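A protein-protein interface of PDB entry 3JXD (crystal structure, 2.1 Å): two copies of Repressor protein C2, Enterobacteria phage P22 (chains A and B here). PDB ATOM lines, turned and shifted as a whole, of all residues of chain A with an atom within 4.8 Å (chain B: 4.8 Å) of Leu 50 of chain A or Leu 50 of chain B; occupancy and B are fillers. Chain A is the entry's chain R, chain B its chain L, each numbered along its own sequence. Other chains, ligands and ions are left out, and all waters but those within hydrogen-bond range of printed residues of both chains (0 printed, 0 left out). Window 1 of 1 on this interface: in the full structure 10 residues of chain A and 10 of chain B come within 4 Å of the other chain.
OD1 of Asp 61 of chain A lies within salt-bridge range of NZ of Lys 54 of chain B (3.1 Å). The side-chain amino group (NZ) of Lys 54 of chain A is in salt-bridge range of the side-chain carboxylate (OD1) of Asp 61 of chain B (2.6 Å). The backbone NH (N) of Gly 46 of chain A lies close to the backbone NH (N) of Gly 46 of chain B, 3.5 Å away.
OG of Ser 53 of chain A lies within hydrogen-bond range of O of Leu 50 of chain A (3.1 Å). OG of Ser 53 of chain B lies within hydrogen-bond range of O of Leu 50 of chain B.
Among the printed residues, pairs that only touch across the chains: Gly 46 of chain A with Leu 49 of chain B (3.6 Å), Leu 50 of chain A with Asp 61 of chain B (3.7 Å), Leu 49 of chain A with Gly 46 of chain B (3.7 Å), Pro 60 of chain A with Leu 50 of chain B (3.7 Å), Leu 50 of chain A with Pro 60 of chain B (3.7 Å), Asp 61 of chain A with Leu 50 of chain B (3.8 Å), Leu 64 of chain A with Glu 47 of chain B (3.8 Å), Leu 50 of chain A with Leu 50 of chain B (3.8 Å), Leu 50 of chain A with Leu 64 of chain B (3.8 Å), Leu 64 of chain A with Leu 50 of chain B (3.9 Å), Glu 47 of chain A with Leu 64 of chain B (3.9 Å), Leu 50 of chain A with Leu 49 of chain B (3.9 Å) and Leu 49 of chain A with Leu 50 of chain B (3.96 Å).
Of chain B, only Leu 49, Leu 50, Pro 60, Asp 61 and Leu 64 come within 4 Å of Leu 50 of chain A. Leu 50 of chain B touches just these residues of chain A: Leu 49, Leu 50, Pro 60, Asp 61 and Leu 64. Of the printed residues of chain A, Leu 64 of chain B touches Glu 47 and Leu 50. Of the printed residues of chain B, Leu 49 of chain A touches Gly 46 and Leu 50. Printed residues of chain A within 4 Å of Pro 60 of chain B: Leu 50.
Printed residues of chain B that touch a printed residue of chain A: Gly 46, Glu 47, Leu 49, Leu 50, Lys 54, Pro 60, Asp 61 and Leu 64. Hydrophobic or aromatic side chains of chain B that line the printed part of chain A: Leu 49, Leu 50, Pro 60 and Leu 64. Along chain B the printed residues that touch a printed residue of chain A span positions 46 to 64. Hydrophobic or aromatic side chains of chain A within 4 Å of the printed part of chain B: Leu 49, Leu 50, Pro 60 and Leu 64. Along chain A the printed residues that touch a printed residue of chain B span positions 46 to 64. Among the printed residues, Asp or Glu carboxylates within 4 Å of a Lys or Arg side-chain nitrogen of the other chain: Lys 54 of chain A with Asp 61 of chain B (2.6 Å) and Asp 61 of chain A with Lys 54 of chain B (3.1 Å).
Leu 49 of chain A touches Leu 50 of chain B, and with the chains exchanged Leu 50 of chain A touches Leu 49 of chain B. Leu 50 of chain A touches Pro 60 of chain B, and with the chains exchanged Pro 60 of chain A touches Leu 50 of chain B. Leu 50 of chain A touches Asp 61 of chain B, and with the chains exchanged Asp 61 of chain A touches Leu 50 of chain B. Leu 50 of chain A touches Leu 64 of chain B, and with the chains exchanged Leu 64 of chain A touches Leu 50 of chain B. Of the 16 pairs that touch across the chains among the printed residues, 16 have their exchanged pair printed and touching as well.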
ATOM      1  N   GLY A  46     -16.699  21.496  13.506  1.00  0.00           N
ATOM      2  CA  GLY A  46     -17.420  22.717  13.873  1.00  0.00           C
ATOM      3  C   GLY A  46     -17.871  23.505  12.666  1.00  0.00           C
ATOM      4  O   GLY A  46     -19.061  23.829  12.534  1.00  0.00           O
ATOM      5  N   GLU A  47     -16.947  23.737  11.728  1.00  0.00           N
ATOM      6  CA  GLU A  47     -17.273  24.413  10.499  1.00  0.00           C
ATOM      7  C   GLU A  47     -18.334  23.645   9.676  1.00  0.00           C
ATOM      8  O   GLU A  47     -19.285  24.254   9.151  1.00  0.00           O
ATOM      9  CB  GLU A  47     -15.988  24.596   9.643  1.00  0.00           C
ATOM     10  CG  GLU A  47     -16.288  24.890   8.216  1.00  0.00           C
ATOM     11  CD  GLU A  47     -15.031  25.297   7.439  1.00  0.00           C
ATOM     12  OE1 GLU A  47     -15.144  26.202   6.587  1.00  0.00           O
ATOM     13  OE2 GLU A  47     -13.950  24.722   7.694  1.00  0.00           O
ATOM     14  N   ASN A  48     -18.203  22.320   9.600  1.00  0.00           N
ATOM     15  CA  ASN A  48     -19.191  21.513   8.829  1.00  0.00           C
ATOM     16  C   ASN A  48     -20.565  21.406   9.497  1.00  0.00           C
ATOM     17  O   ASN A  48     -21.587  21.329   8.821  1.00  0.00           O
ATOM     18  CB  ASN A  48     -18.642  20.126   8.478  1.00  0.00           C
ATOM     19  CG  ASN A  48     -17.473  20.197   7.505  1.00  0.00           C
ATOM     20  OD1 ASN A  48     -17.346  21.171   6.744  1.00  0.00           O
ATOM     21  ND2 ASN A  48     -16.631  19.192   7.522  1.00  0.00           N
ATOM     22  N   LEU A  49     -20.579  21.350  10.818  1.00  0.00           N
ATOM     23  CA  LEU A  49     -21.839  21.348  11.567  1.00  0.00           C
ATOM     24  C   LEU A  49     -22.637  22.635  11.240  1.00  0.00           C
ATOM     25  O   LEU A  49     -23.842  22.594  10.938  1.00  0.00           O
ATOM     26  CB  LEU A  49     -21.593  21.263  13.088  1.00  0.00           C
ATOM     27  CG  LEU A  49     -22.918  21.281  13.927  1.00  0.00           C
ATOM     28  CD1 LEU A  49     -23.917  20.181  13.457  1.00  0.00           C
ATOM     29  CD2 LEU A  49     -22.647  21.136  15.378  1.00  0.00           C
ATOM     30  N   LEU A  50     -21.950  23.757  11.286  1.00  0.00           N
ATOM     31  CA  LEU A  50     -22.581  25.037  10.943  1.00  0.00           C
ATOM     32  C   LEU A  50     -23.081  25.096   9.529  1.00  0.00           C
ATOM     33  O   LEU A  50     -24.216  25.537   9.326  1.00  0.00           O
ATOM     34  CB  LEU A  50     -21.750  26.262  11.323  1.00  0.00           C
ATOM     35  CG  LEU A  50     -21.912  26.728  12.787  1.00  0.00           C
ATOM     36  CD1 LEU A  50     -23.257  27.481  12.879  1.00  0.00           C
ATOM     37  CD2 LEU A  50     -21.902  25.589  13.880  1.00  0.00           C
ATOM     38  N   ALA A  51     -22.296  24.616   8.562  1.00  0.00           N
ATOM     39  CA  ALA A  51     -22.780  24.563   7.184  1.00  0.00           C
ATOM     40  C   ALA A  51     -23.912  23.595   6.972  1.00  0.00           C
ATOM     41  O   ALA A  51     -24.847  23.855   6.167  1.00  0.00           O
ATOM     42  CB  ALA A  51     -21.619  24.271   6.201  1.00  0.00           C
ATOM     43  N   LEU A  52     -23.839  22.449   7.659  1.00  0.00           N
ATOM     44  CA  LEU A  52     -24.917  21.490   7.606  1.00  0.00           C
ATOM     45  C   LEU A  52     -26.256  22.050   8.151  1.00  0.00           C
ATOM     46  O   LEU A  52     -27.327  21.813   7.590  1.00  0.00           O
ATOM     47  CB  LEU A  52     -24.545  20.233   8.389  1.00  0.00           C
ATOM     48  CG  LEU A  52     -25.576  19.104   8.439  1.00  0.00           C
ATOM     49  CD1 LEU A  52     -25.989  18.487   7.030  1.00  0.00           C
ATOM     50  CD2 LEU A  52     -25.104  18.026   9.421  1.00  0.00           C
ATOM     51  N   SER A  53     -26.190  22.721   9.280  1.00  0.00           N
ATOM     52  CA  SER A  53     -27.426  23.173   9.920  1.00  0.00           C
ATOM     53  C   SER A  53     -28.129  24.226   9.015  1.00  0.00           C
ATOM     54  O   SER A  53     -29.322  24.156   8.842  1.00  0.00           O
ATOM     55  CB  SER A  53     -27.136  23.635  11.363  1.00  0.00           C
ATOM     56  OG  SER A  53     -26.491  24.882  11.323  1.00  0.00           O
ATOM     57  N   LYS A  54     -27.356  25.086   8.351  1.00  0.00           N
ATOM     58  CA  LYS A  54     -27.868  25.990   7.316  1.00  0.00           C
ATOM     59  C   LYS A  54     -28.485  25.284   6.117  1.00  0.00           C
ATOM     60  O   LYS A  54     -29.622  25.610   5.739  1.00  0.00           O
ATOM     61  CB  LYS A  54     -26.784  26.939   6.833  1.00  0.00           C
ATOM     62  CG  LYS A  54     -26.348  27.838   7.958  1.00  0.00           C
ATOM     63  CD  LYS A  54     -25.492  28.961   7.502  1.00  0.00           C
ATOM     64  CE  LYS A  54     -25.112  29.778   8.719  1.00  0.00           C
ATOM     65  NZ  LYS A  54     -23.906  29.227   9.388  1.00  0.00           N
ATOM     66  N   PRO A  60     -27.792  24.233  14.903  1.00  0.00           N
ATOM     67  CA  PRO A  60     -26.788  23.235  15.315  1.00  0.00           C
ATOM     68  C   PRO A  60     -27.200  22.477  16.571  1.00  0.00           C
ATOM     69  O   PRO A  60     -26.944  21.315  16.698  1.00  0.00           O
ATOM     70  CB  PRO A  60     -25.494  24.064  15.543  1.00  0.00           C
ATOM     71  CG  PRO A  60     -25.711  25.420  14.934  1.00  0.00           C
ATOM     72  CD  PRO A  60     -27.227  25.584  14.681  1.00  0.00           C
ATOM     73  N   ASP A  61     -27.895  23.139  17.489  1.00  0.00           N
ATOM     74  CA  ASP A  61     -28.308  22.493  18.723  1.00  0.00           C
ATOM     75  C   ASP A  61     -29.314  21.395  18.494  1.00  0.00           C
ATOM     76  O   ASP A  61     -29.217  20.296  19.079  1.00  0.00           O
ATOM     77  CB  ASP A  61     -28.822  23.541  19.711  1.00  0.00           C
ATOM     78  CG  ASP A  61     -27.684  24.268  20.370  1.00  0.00           C
ATOM     79  OD1 ASP A  61     -27.589  25.495  20.212  1.00  0.00           O
ATOM     80  OD2 ASP A  61     -26.839  23.572  20.985  1.00  0.00           O
ATOM     81  N   LEU A  64     -27.458  18.439  17.186  1.00  0.00           N
ATOM     82  CA  LEU A  64     -26.616  17.862  18.219  1.00  0.00           C
ATOM     83  C   LEU A  64     -27.368  17.199  19.360  1.00  0.00           C
ATOM     84  O   LEU A  64     -26.983  16.128  19.788  1.00  0.00           O
ATOM     85  CB  LEU A  64     -25.753  18.930  18.832  1.00  0.00           C
ATOM     86  CG  LEU A  64     -24.384  19.221  18.254  1.00  0.00           C
ATOM     87  CD1 LEU A  64     -23.801  20.355  19.072  1.00  0.00           C
ATOM     88  CD2 LEU A  64     -23.511  17.960  18.331  1.00  0.00           C
ATOM     89  N   GLY B  46     -17.795  19.814  16.316  1.00  0.00           N
ATOM     90  CA  GLY B  46     -19.167  20.346  16.276  1.00  0.00           C
ATOM     91  C   GLY B  46     -19.715  20.582  17.682  1.00  0.00           C
ATOM     92  O   GLY B  46     -20.108  21.697  18.008  1.00  0.00           O
ATOM     93  N   GLU B  47     -19.677  19.540  18.511  1.00  0.00           N
ATOM     94  CA  GLU B  47     -20.176  19.614  19.871  1.00  0.00           C
ATOM     95  C   GLU B  47     -19.402  20.639  20.718  1.00  0.00           C
ATOM     96  O   GLU B  47     -19.998  21.473  21.428  1.00  0.00           O
ATOM     97  CB  GLU B  47     -20.106  18.211  20.500  1.00  0.00           C
ATOM     98  CG  GLU B  47     -20.115  18.255  21.999  1.00  0.00           C
ATOM     99  CD  GLU B  47     -20.517  16.933  22.630  1.00  0.00           C
ATOM    100  OE1 GLU B  47     -20.617  15.913  21.906  1.00  0.00           O
ATOM    101  OE2 GLU B  47     -20.748  16.924  23.858  1.00  0.00           O
ATOM    102  N   ASN B  48     -18.062  20.628  20.586  1.00  0.00           N
ATOM    103  CA  ASN B  48     -17.214  21.571  21.279  1.00  0.00           C
ATOM    104  C   ASN B  48     -17.388  22.985  20.795  1.00  0.00           C
ATOM    105  O   ASN B  48     -17.329  23.938  21.643  1.00  0.00           O
ATOM    106  CB  ASN B  48     -15.709  21.134  21.321  1.00  0.00           C
ATOM    107  CG  ASN B  48     -15.507  19.856  22.123  1.00  0.00           C
ATOM    108  OD1 ASN B  48     -16.318  19.529  23.011  1.00  0.00           O
ATOM    109  ND2 ASN B  48     -14.435  19.129  21.836  1.00  0.00           N
ATOM    110  N   LEU B  49     -17.606  23.183  19.491  1.00  0.00           N
ATOM    111  CA  LEU B  49     -17.773  24.552  19.044  1.00  0.00           C
ATOM    112  C   LEU B  49     -19.052  25.163  19.710  1.00  0.00           C
ATOM    113  O   LEU B  49     -19.074  26.329  20.074  1.00  0.00           O
ATOM    114  CB  LEU B  49     -17.907  24.677  17.555  1.00  0.00           C
ATOM    115  CG  LEU B  49     -18.214  26.070  16.936  1.00  0.00           C
ATOM    116  CD1 LEU B  49     -17.193  27.164  17.271  1.00  0.00           C
ATOM    117  CD2 LEU B  49     -18.323  25.909  15.417  1.00  0.00           C
ATOM    118  N   LEU B  50     -20.111  24.376  19.755  1.00  0.00           N
ATOM    119  CA  LEU B  50     -21.381  24.852  20.318  1.00  0.00           C
ATOM    120  C   LEU B  50     -21.238  25.131  21.800  1.00  0.00           C
ATOM    121  O   LEU B  50     -21.697  26.176  22.246  1.00  0.00           O
ATOM    122  CB  LEU B  50     -22.531  23.886  20.019  1.00  0.00           C
ATOM    123  CG  LEU B  50     -23.271  24.307  18.728  1.00  0.00           C
ATOM    124  CD1 LEU B  50     -24.067  25.620  18.904  1.00  0.00           C
ATOM    125  CD2 LEU B  50     -22.394  24.466  17.503  1.00  0.00           C
ATOM    126  N   ALA B  51     -20.582  24.223  22.532  1.00  0.00           N
ATOM    127  CA  ALA B  51     -20.343  24.420  23.965  1.00  0.00           C
ATOM    128  C   ALA B  51     -19.463  25.643  24.225  1.00  0.00           C
ATOM    129  O   ALA B  51     -19.698  26.416  25.152  1.00  0.00           O
ATOM    130  CB  ALA B  51     -19.808  23.156  24.646  1.00  0.00           C
ATOM    131  N   LEU B  52     -18.470  25.844  23.366  1.00  0.00           N
ATOM    132  CA  LEU B  52     -17.607  26.999  23.451  1.00  0.00           C
ATOM    133  C   LEU B  52     -18.375  28.328  23.249  1.00  0.00           C
ATOM    134  O   LEU B  52     -18.118  29.316  23.941  1.00  0.00           O
ATOM    135  CB  LEU B  52     -16.499  26.915  22.393  1.00  0.00           C
ATOM    136  CG  LEU B  52     -15.574  28.105  22.276  1.00  0.00           C
ATOM    137  CD1 LEU B  52     -14.791  28.240  23.616  1.00  0.00           C
ATOM    138  CD2 LEU B  52     -14.701  27.871  21.019  1.00  0.00           C
ATOM    139  N   SER B  53     -19.229  28.349  22.241  1.00  0.00           N
ATOM    140  CA  SER B  53     -20.007  29.542  21.947  1.00  0.00           C
ATOM    141  C   SER B  53     -20.960  29.934  23.120  1.00  0.00           C
ATOM    142  O   SER B  53     -21.068  31.116  23.427  1.00  0.00           O
ATOM    143  CB  SER B  53     -20.749  29.384  20.610  1.00  0.00           C
ATOM    144  OG  SER B  53     -21.834  28.501  20.783  1.00  0.00           O
ATOM    145  N   LYS B  54     -21.601  28.961  23.769  1.00  0.00           N
ATOM    146  CA  LYS B  54     -22.398  29.185  25.015  1.00  0.00           C
ATOM    147  C   LYS B  54     -21.561  29.725  26.180  1.00  0.00           C
ATOM    148  O   LYS B  54     -21.907  30.751  26.758  1.00  0.00           O
ATOM    149  CB  LYS B  54     -23.140  27.940  25.430  1.00  0.00           C
ATOM    150  CG  LYS B  54     -24.089  27.541  24.331  1.00  0.00           C
ATOM    151  CD  LYS B  54     -24.894  26.330  24.654  1.00  0.00           C
ATOM    152  CE  LYS B  54     -25.841  25.991  23.458  1.00  0.00           C
ATOM    153  NZ  LYS B  54     -25.251  26.334  22.119  1.00  0.00           N
ATOM    154  N   PRO B  60     -21.864  30.619  17.255  1.00  0.00           N
ATOM    155  CA  PRO B  60     -20.857  29.780  16.545  1.00  0.00           C
ATOM    156  C   PRO B  60     -20.339  30.473  15.288  1.00  0.00           C
ATOM    157  O   PRO B  60     -19.153  30.388  15.006  1.00  0.00           O
ATOM    158  CB  PRO B  60     -21.624  28.515  16.180  1.00  0.00           C
ATOM    159  CG  PRO B  60     -22.849  28.458  17.088  1.00  0.00           C
ATOM    160  CD  PRO B  60     -23.144  29.904  17.476  1.00  0.00           C
ATOM    161  N   ASP B  61     -21.224  31.163  14.561  1.00  0.00           N
ATOM    162  CA  ASP B  61     -20.857  31.896  13.335  1.00  0.00           C
ATOM    163  C   ASP B  61     -19.884  33.046  13.582  1.00  0.00           C
ATOM    164  O   ASP B  61     -18.972  33.277  12.787  1.00  0.00           O
ATOM    165  CB  ASP B  61     -22.098  32.443  12.654  1.00  0.00           C
ATOM    166  CG  ASP B  61     -23.112  31.357  12.344  1.00  0.00           C
ATOM    167  OD1 ASP B  61     -22.994  30.768  11.262  1.00  0.00           O
ATOM    168  OD2 ASP B  61     -23.997  31.089  13.215  1.00  0.00           O
ATOM    169  N   LEU B  64     -16.470  31.390  14.100  1.00  0.00           N
ATOM    170  CA  LEU B  64     -15.889  30.770  12.903  1.00  0.00           C
ATOM    171  C   LEU B  64     -15.524  31.819  11.880  1.00  0.00           C
ATOM    172  O   LEU B  64     -14.433  31.774  11.287  1.00  0.00           O
ATOM    173  CB  LEU B  64     -16.899  29.831  12.268  1.00  0.00           C
ATOM    174  CG  LEU B  64     -17.014  28.400  12.758  1.00  0.00           C
ATOM    175  CD1 LEU B  64     -18.284  27.820  12.110  1.00  0.00           C
ATOM    176  CD2 LEU B  64     -15.755  27.598  12.376  1.00  0.00           C
